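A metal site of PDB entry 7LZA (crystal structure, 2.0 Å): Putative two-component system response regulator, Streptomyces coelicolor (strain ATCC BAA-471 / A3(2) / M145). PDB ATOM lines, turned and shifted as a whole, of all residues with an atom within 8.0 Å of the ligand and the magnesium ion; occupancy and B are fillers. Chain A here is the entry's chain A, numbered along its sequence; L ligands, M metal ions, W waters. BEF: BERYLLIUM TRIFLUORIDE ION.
OD1 of Asp 52 lies close to NZ of Lys 102 (3.6 Å).
The backbone carbonyl oxygen (O) of Val 7 is in hydrogen-bond range of the backbone NH (N) of Asp 52, at 2.8 Å.
The backbone NH (N) of Lys 102 is in hydrogen-bond range of the backbone carbonyl oxygen (O) of Thr 80 (3.0 Å).
OG1 of Thr 80 sits at hydrogen-bond distance from N of Ala 82, at 3.1 Å.
O of Leu 100 sits at hydrogen-bond distance from N of Thr 80, 3.1 Å away.
The side-chain carboxylate of Glu 8 is in salt-bridge range of the side-chain amino group of Lys 102 (2.7 Å).
The guanidinium group (NE) of Arg 53 is in salt-bridge range of the side-chain carboxylate (OD1) of Asp 61 (2.8 Å).
The backbone carbonyl oxygen of Arg 53 sits at hydrogen-bond distance from the backbone NH of Gly 60 (3.0 Å).
The side-chain carboxylate (OD1) of Asp 52 binds a beryllium atom (BE) of the ligand, 1.4 Å away.
N of Asp 54 is in hydrogen-bond range of F2 of the ligand, 3.1 Å away.
The side-chain hydroxyl (OG1) of Thr 80 sits at hydrogen-bond distance from a fluorine (F2) of the ligand, at 2.5 Å.
A fluorine (F3) of the ligand lies within hydrogen-bond range of the backbone NH (N) of Ala 81 (2.9 Å).
A fluorine (F3) of the ligand sits at hydrogen-bond distance from the side-chain amino group (NZ) of Lys 102, at 2.9 Å.
N of Arg 53 is in hydrogen-bond range of F2 of the ligand (3.1 Å).
Within 4 Å of the ligand: Asp 52, Arg 53, Asp 54, Thr 80, Ala 81 and Lys 102.
Along chain A the residues within 4 Å of the ligand span positions 52 to 102.
OD2 of Asp 52 binds the magnesium ion (2.0 Å).
A fluorine (F1) of the ligand is bound to the magnesium ion (2.0 Å).
The magnesium ion is bound by water W4 (2.0 Å).
The magnesium ion is bound by OD2 of Asp 9 (2.1 Å).
The magnesium ion is bound by the backbone carbonyl oxygen (O) of Asp 54 (2.1 Å).
Water W3 binds the magnesium ion.
Water W4 lies within hydrogen-bond range of OE1 of Glu 8 and NZ of Lys 102.
Three residues have an atom within 4 Å of the magnesium ion: Asp 9, Asp 52 and Asp 54.
The nearest printed residue that does not touch the magnesium ion is Glu 8 (4.03 Å).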
ATOM      1  N   VAL A   7       1.521  25.491  19.071  1.00  0.00           N
ATOM      2  CA  VAL A   7       0.715  25.000  20.178  1.00  0.00           C
ATOM      3  C   VAL A   7       0.601  26.128  21.184  1.00  0.00           C
ATOM      4  O   VAL A   7       1.581  26.472  21.863  1.00  0.00           O
ATOM      5  CB  VAL A   7       1.335  23.754  20.823  1.00  0.00           C
ATOM      6  CG1 VAL A   7       0.413  23.252  21.902  1.00  0.00           C
ATOM      7  CG2 VAL A   7       1.571  22.676  19.781  1.00  0.00           C
ATOM      8  N   GLU A   8      -0.591  26.726  21.270  1.00  0.00           N
ATOM      9  CA  GLU A   8      -0.801  27.929  22.086  1.00  0.00           C
ATOM     10  C   GLU A   8      -2.281  28.023  22.416  1.00  0.00           C
ATOM     11  O   GLU A   8      -3.112  27.945  21.506  1.00  0.00           O
ATOM     12  CB  GLU A   8      -0.358  29.169  21.311  1.00  0.00           C
ATOM     13  CG  GLU A   8      -0.913  30.462  21.861  1.00  0.00           C
ATOM     14  CD  GLU A   8      -0.385  30.755  23.268  1.00  0.00           C
ATOM     15  OE1 GLU A   8      -1.202  30.955  24.192  1.00  0.00           O
ATOM     16  OE2 GLU A   8       0.855  30.775  23.436  1.00  0.00           O
ATOM     17  N   ASP A   9      -2.625  28.208  23.704  1.00  0.00           N
ATOM     18  CA  ASP A   9      -4.017  28.129  24.117  1.00  0.00           C
ATOM     19  C   ASP A   9      -4.731  29.478  24.170  1.00  0.00           C
ATOM     20  O   ASP A   9      -5.950  29.499  24.363  1.00  0.00           O
ATOM     21  CB  ASP A   9      -4.154  27.420  25.481  1.00  0.00           C
ATOM     22  CG  ASP A   9      -3.438  28.133  26.627  1.00  0.00           C
ATOM     23  OD1 ASP A   9      -3.955  28.133  27.763  1.00  0.00           O
ATOM     24  OD2 ASP A   9      -2.343  28.681  26.399  1.00  0.00           O
ATOM     25  N   GLU A  10      -4.034  30.606  23.972  1.00  0.00           N
ATOM     26  CA  GLU A  10      -4.724  31.882  23.824  1.00  0.00           C
ATOM     27  C   GLU A  10      -5.014  32.100  22.344  1.00  0.00           C
ATOM     28  O   GLU A  10      -4.075  32.287  21.567  1.00  0.00           O
ATOM     29  CB  GLU A  10      -3.880  33.020  24.403  1.00  0.00           C
ATOM     30  CG  GLU A  10      -4.680  34.315  24.672  1.00  0.00           C
ATOM     31  CD  GLU A  10      -5.124  35.035  23.384  1.00  0.00           C
ATOM     32  OE1 GLU A  10      -6.297  34.900  22.975  1.00  0.00           O
ATOM     33  OE2 GLU A  10      -4.274  35.741  22.775  1.00  0.00           O
ATOM     34  N   LEU A  13      -3.849  35.272  19.984  1.00  0.00           N
ATOM     35  CA  LEU A  13      -2.399  35.289  19.794  1.00  0.00           C
ATOM     36  C   LEU A  13      -1.969  34.254  18.760  1.00  0.00           C
ATOM     37  O   LEU A  13      -1.189  34.554  17.863  1.00  0.00           O
ATOM     38  CB  LEU A  13      -1.680  35.027  21.122  1.00  0.00           C
ATOM     39  CG  LEU A  13      -0.179  34.753  21.053  1.00  0.00           C
ATOM     40  CD1 LEU A  13       0.500  35.956  20.468  1.00  0.00           C
ATOM     41  CD2 LEU A  13       0.399  34.473  22.457  1.00  0.00           C
ATOM     42  N   GLY A  32      -4.864  24.359  20.039  1.00  0.00           N
ATOM     43  CA  GLY A  32      -5.188  25.039  21.284  1.00  0.00           C
ATOM     44  C   GLY A  32      -4.984  24.227  22.550  1.00  0.00           C
ATOM     45  O   GLY A  32      -5.117  24.778  23.635  1.00  0.00           O
ATOM     46  N   LEU A  51       6.081  25.853  20.877  1.00  0.00           N
ATOM     47  CA  LEU A  51       5.311  25.287  21.986  1.00  0.00           C
ATOM     48  C   LEU A  51       5.159  26.289  23.111  1.00  0.00           C
ATOM     49  O   LEU A  51       6.157  26.704  23.730  1.00  0.00           O
ATOM     50  CB  LEU A  51       5.987  24.023  22.514  1.00  0.00           C
ATOM     51  CG  LEU A  51       6.212  22.892  21.505  1.00  0.00           C
ATOM     52  CD1 LEU A  51       6.845  21.697  22.214  1.00  0.00           C
ATOM     53  CD2 LEU A  51       4.886  22.492  20.912  1.00  0.00           C
ATOM     54  N   ASP A  52       3.924  26.657  23.402  1.00  0.00           N
ATOM     55  CA  ASP A  52       3.542  27.177  24.714  1.00  0.00           C
ATOM     56  C   ASP A  52       3.679  26.085  25.770  1.00  0.00           C
ATOM     57  O   ASP A  52       3.496  24.893  25.479  1.00  0.00           O
ATOM     58  CB  ASP A  52       2.103  27.682  24.658  1.00  0.00           C
ATOM     59  CG  ASP A  52       1.670  28.465  25.893  1.00  0.00           C
ATOM     60  OD1 ASP A  52       2.510  29.027  26.645  1.00  0.00           O
ATOM     61  OD2 ASP A  52       0.435  28.559  26.076  1.00  0.00           O
ATOM     62  N   ARG A  53       3.977  26.475  26.998  1.00  0.00           N
ATOM     63  CA  ARG A  53       4.149  25.466  28.043  1.00  0.00           C
ATOM     64  C   ARG A  53       2.850  25.158  28.797  1.00  0.00           C
ATOM     65  O   ARG A  53       2.507  23.985  28.990  1.00  0.00           O
ATOM     66  CB  ARG A  53       5.246  25.890  29.025  1.00  0.00           C
ATOM     67  CG  ARG A  53       6.609  25.920  28.359  1.00  0.00           C
ATOM     68  CD  ARG A  53       7.723  26.178  29.380  1.00  0.00           C
ATOM     69  NE  ARG A  53       8.124  24.957  30.055  1.00  0.00           N
ATOM     70  CZ  ARG A  53       9.216  24.854  30.812  1.00  0.00           C
ATOM     71  NH1 ARG A  53      10.003  25.919  30.973  1.00  0.00           N
ATOM     72  NH2 ARG A  53       9.527  23.706  31.380  1.00  0.00           N
ATOM     73  N   ASP A  54       2.109  26.186  29.176  1.00  0.00           N
ATOM     74  CA  ASP A  54       0.879  26.016  29.954  1.00  0.00           C
ATOM     75  C   ASP A  54      -0.317  26.020  29.002  1.00  0.00           C
ATOM     76  O   ASP A  54      -0.739  27.069  28.509  1.00  0.00           O
ATOM     77  CB  ASP A  54       0.759  27.121  31.009  1.00  0.00           C
ATOM     78  CG  ASP A  54      -0.519  27.013  31.818  1.00  0.00           C
ATOM     79  OD1 ASP A  54      -1.102  25.914  31.895  1.00  0.00           O
ATOM     80  OD2 ASP A  54      -0.933  28.045  32.391  1.00  0.00           O
ATOM     81  N   ILE A  55      -0.837  24.831  28.719  1.00  0.00           N
ATOM     82  CA  ILE A  55      -1.982  24.613  27.845  1.00  0.00           C
ATOM     83  C   ILE A  55      -2.886  23.551  28.461  1.00  0.00           C
ATOM     84  O   ILE A  55      -2.436  22.732  29.269  1.00  0.00           O
ATOM     85  CB  ILE A  55      -1.544  24.153  26.439  1.00  0.00           C
ATOM     86  CG1 ILE A  55      -0.814  22.818  26.525  1.00  0.00           C
ATOM     87  CG2 ILE A  55      -0.645  25.207  25.770  1.00  0.00           C
ATOM     88  CD1 ILE A  55      -0.366  22.291  25.173  1.00  0.00           C
ATOM     89  N   PRO A  56      -4.161  23.540  28.090  1.00  0.00           N
ATOM     90  CA  PRO A  56      -5.065  22.460  28.536  1.00  0.00           C
ATOM     91  C   PRO A  56      -4.609  21.108  28.022  1.00  0.00           C
ATOM     92  O   PRO A  56      -4.019  20.983  26.942  1.00  0.00           O
ATOM     93  CB  PRO A  56      -6.423  22.847  27.926  1.00  0.00           C
ATOM     94  CG  PRO A  56      -6.334  24.281  27.639  1.00  0.00           C
ATOM     95  CD  PRO A  56      -4.893  24.623  27.409  1.00  0.00           C
ATOM     96  N   GLY A  60       2.662  21.594  27.191  1.00  0.00           N
ATOM     97  CA  GLY A  60       3.697  21.814  26.193  1.00  0.00           C
ATOM     98  C   GLY A  60       4.970  21.040  26.497  1.00  0.00           C
ATOM     99  O   GLY A  60       5.649  20.591  25.578  1.00  0.00           O
ATOM    100  N   ASP A  61       5.301  20.869  27.783  1.00  0.00           N
ATOM    101  CA  ASP A  61       6.462  20.073  28.186  1.00  0.00           C
ATOM    102  C   ASP A  61       6.297  18.610  27.769  1.00  0.00           C
ATOM    103  O   ASP A  61       7.255  17.988  27.272  1.00  0.00           O
ATOM    104  CB  ASP A  61       6.676  20.153  29.692  1.00  0.00           C
ATOM    105  CG  ASP A  61       6.981  21.568  30.165  1.00  0.00           C
ATOM    106  OD1 ASP A  61       6.954  22.494  29.324  1.00  0.00           O
ATOM    107  OD2 ASP A  61       7.239  21.762  31.384  1.00  0.00           O
ATOM    108  N   MET A  78      10.335  26.879  22.328  1.00  0.00           N
ATOM    109  CA  MET A  78       9.330  27.158  23.330  1.00  0.00           C
ATOM    110  C   MET A  78       9.072  28.663  23.368  1.00  0.00           C
ATOM    111  O   MET A  78       9.996  29.460  23.256  1.00  0.00           O
ATOM    112  CB  MET A  78       9.761  26.621  24.699  1.00  0.00           C
ATOM    113  CG  MET A  78       9.716  25.070  24.775  1.00  0.00           C
ATOM    114  SD  MET A  78      10.180  24.604  26.459  1.00  0.00           S
ATOM    115  CE  MET A  78       9.909  22.808  26.462  1.00  0.00           C
ATOM    116  N   LEU A  79       7.796  29.027  23.425  1.00  0.00           N
ATOM    117  CA  LEU A  79       7.351  30.409  23.331  1.00  0.00           C
ATOM    118  C   LEU A  79       6.361  30.591  24.476  1.00  0.00           C
ATOM    119  O   LEU A  79       5.227  30.118  24.383  1.00  0.00           O
ATOM    120  CB  LEU A  79       6.701  30.688  21.965  1.00  0.00           C
ATOM    121  CG  LEU A  79       6.059  32.065  21.751  1.00  0.00           C
ATOM    122  CD1 LEU A  79       7.068  33.150  21.995  1.00  0.00           C
ATOM    123  CD2 LEU A  79       5.483  32.191  20.339  1.00  0.00           C
ATOM    124  N   THR A  80       6.777  31.251  25.559  1.00  0.00           N
ATOM    125  CA  THR A  80       6.058  31.029  26.801  1.00  0.00           C
ATOM    126  C   THR A  80       6.244  32.200  27.765  1.00  0.00           C
ATOM    127  O   THR A  80       7.273  32.890  27.733  1.00  0.00           O
ATOM    128  CB  THR A  80       6.519  29.725  27.477  1.00  0.00           C
ATOM    129  OG1 THR A  80       5.906  29.601  28.767  1.00  0.00           O
ATOM    130  CG2 THR A  80       8.035  29.714  27.640  1.00  0.00           C
ATOM    131  N   ALA A  81       5.243  32.393  28.625  1.00  0.00           N
ATOM    132  CA  ALA A  81       5.311  33.375  29.698  1.00  0.00           C
ATOM    133  C   ALA A  81       6.219  32.936  30.851  1.00  0.00           C
ATOM    134  O   ALA A  81       6.509  33.753  31.744  1.00  0.00           O
ATOM    135  CB  ALA A  81       3.905  33.650  30.224  1.00  0.00           C
ATOM    136  N   ALA A  82       6.653  31.684  30.871  1.00  0.00           N
ATOM    137  CA  ALA A  82       7.528  31.189  31.939  1.00  0.00           C
ATOM    138  C   ALA A  82       8.930  31.698  31.640  1.00  0.00           C
ATOM    139  O   ALA A  82       9.661  31.110  30.838  1.00  0.00           O
ATOM    140  CB  ALA A  82       7.479  29.666  32.022  1.00  0.00           C
ATOM    141  N   ASP A  83       9.302  32.813  32.260  1.00  0.00           N
ATOM    142  CA  ASP A  83      10.484  33.566  31.870  1.00  0.00           C
ATOM    143  C   ASP A  83      11.577  33.593  32.940  1.00  0.00           C
ATOM    144  O   ASP A  83      12.528  34.383  32.813  1.00  0.00           O
ATOM    145  CB  ASP A  83      10.091  34.995  31.504  1.00  0.00           C
ATOM    146  CG  ASP A  83       9.359  35.724  32.627  1.00  0.00           C
ATOM    147  OD1 ASP A  83       9.346  35.218  33.766  1.00  0.00           O
ATOM    148  OD2 ASP A  83       8.770  36.798  32.379  1.00  0.00           O
ATOM    149  N   TYR A  99      14.274  29.105  23.050  1.00  0.00           N
ATOM    150  CA  TYR A  99      13.371  29.443  24.150  1.00  0.00           C
ATOM    151  C   TYR A  99      13.160  30.940  24.069  1.00  0.00           C
ATOM    152  O   TYR A  99      14.104  31.705  24.235  1.00  0.00           O
ATOM    153  CB  TYR A  99      13.968  29.024  25.497  1.00  0.00           C
ATOM    154  CG  TYR A  99      12.990  28.973  26.641  1.00  0.00           C
ATOM    155  CD1 TYR A  99      12.514  30.136  27.243  1.00  0.00           C
ATOM    156  CD2 TYR A  99      12.526  27.753  27.129  1.00  0.00           C
ATOM    157  CE1 TYR A  99      11.616  30.074  28.315  1.00  0.00           C
ATOM    158  CE2 TYR A  99      11.630  27.685  28.172  1.00  0.00           C
ATOM    159  CZ  TYR A  99      11.182  28.840  28.759  1.00  0.00           C
ATOM    160  OH  TYR A  99      10.285  28.742  29.809  1.00  0.00           O
ATOM    161  N   LEU A 100      11.935  31.352  23.758  1.00  0.00           N
ATOM    162  CA  LEU A 100      11.616  32.760  23.561  1.00  0.00           C
ATOM    163  C   LEU A 100      10.513  33.138  24.535  1.00  0.00           C
ATOM    164  O   LEU A 100       9.487  32.467  24.590  1.00  0.00           O
ATOM    165  CB  LEU A 100      11.180  33.006  22.112  1.00  0.00           C
ATOM    166  CG  LEU A 100      11.034  34.435  21.635  1.00  0.00           C
ATOM    167  CD1 LEU A 100      12.401  35.122  21.692  1.00  0.00           C
ATOM    168  CD2 LEU A 100      10.470  34.451  20.187  1.00  0.00           C
ATOM    169  N   THR A 101      10.732  34.196  25.308  1.00  0.00           N
ATOM    170  CA  THR A 101       9.744  34.585  26.309  1.00  0.00           C
ATOM    171  C   THR A 101       8.767  35.628  25.774  1.00  0.00           C
ATOM    172  O   THR A 101       9.094  36.455  24.920  1.00  0.00           O
ATOM    173  CB  THR A 101      10.433  35.137  27.562  1.00  0.00           C
ATOM    174  OG1 THR A 101      11.246  36.263  27.200  1.00  0.00           O
ATOM    175  CG2 THR A 101      11.308  34.061  28.198  1.00  0.00           C
ATOM    176  N   LYS A 102       7.548  35.574  26.314  1.00  0.00           N
ATOM    177  CA  LYS A 102       6.491  36.550  26.108  1.00  0.00           C
ATOM    178  C   LYS A 102       6.661  37.695  27.112  1.00  0.00           C
ATOM    179  O   LYS A 102       6.912  37.452  28.284  1.00  0.00           O
ATOM    180  CB  LYS A 102       5.123  35.909  26.326  1.00  0.00           C
ATOM    181  CG  LYS A 102       4.784  34.753  25.412  1.00  0.00           C
ATOM    182  CD  LYS A 102       3.395  34.201  25.765  1.00  0.00           C
ATOM    183  CE  LYS A 102       3.089  32.893  25.029  1.00  0.00           C
ATOM    184  NZ  LYS A 102       1.760  32.338  25.444  1.00  0.00           N
HETATM  185 BE   BEF L   1       2.373  29.677  27.879  1.00  0.00          BE
HETATM  186  F1  BEF L   1       1.003  29.541  28.556  1.00  0.00           F
HETATM  187  F2  BEF L   1       3.439  28.982  28.794  1.00  0.00           F
HETATM  188  F3  BEF L   1       2.769  31.179  27.870  1.00  0.00           F
HETATM  189 MG    MG M   1      -0.725  28.961  27.661  1.00  0.00          MG
HETATM  190  O   HOH W   1       0.723  32.886  29.160  1.00  0.00           O
HETATM  191  O   HOH W   2       3.425  29.777  31.508  1.00  0.00           O
HETATM  192  O   HOH W   3      -1.921  29.738  29.220  1.00  0.00           O
HETATM  193  O   HOH W   4      -0.762  30.827  26.827  1.00  0.00           O
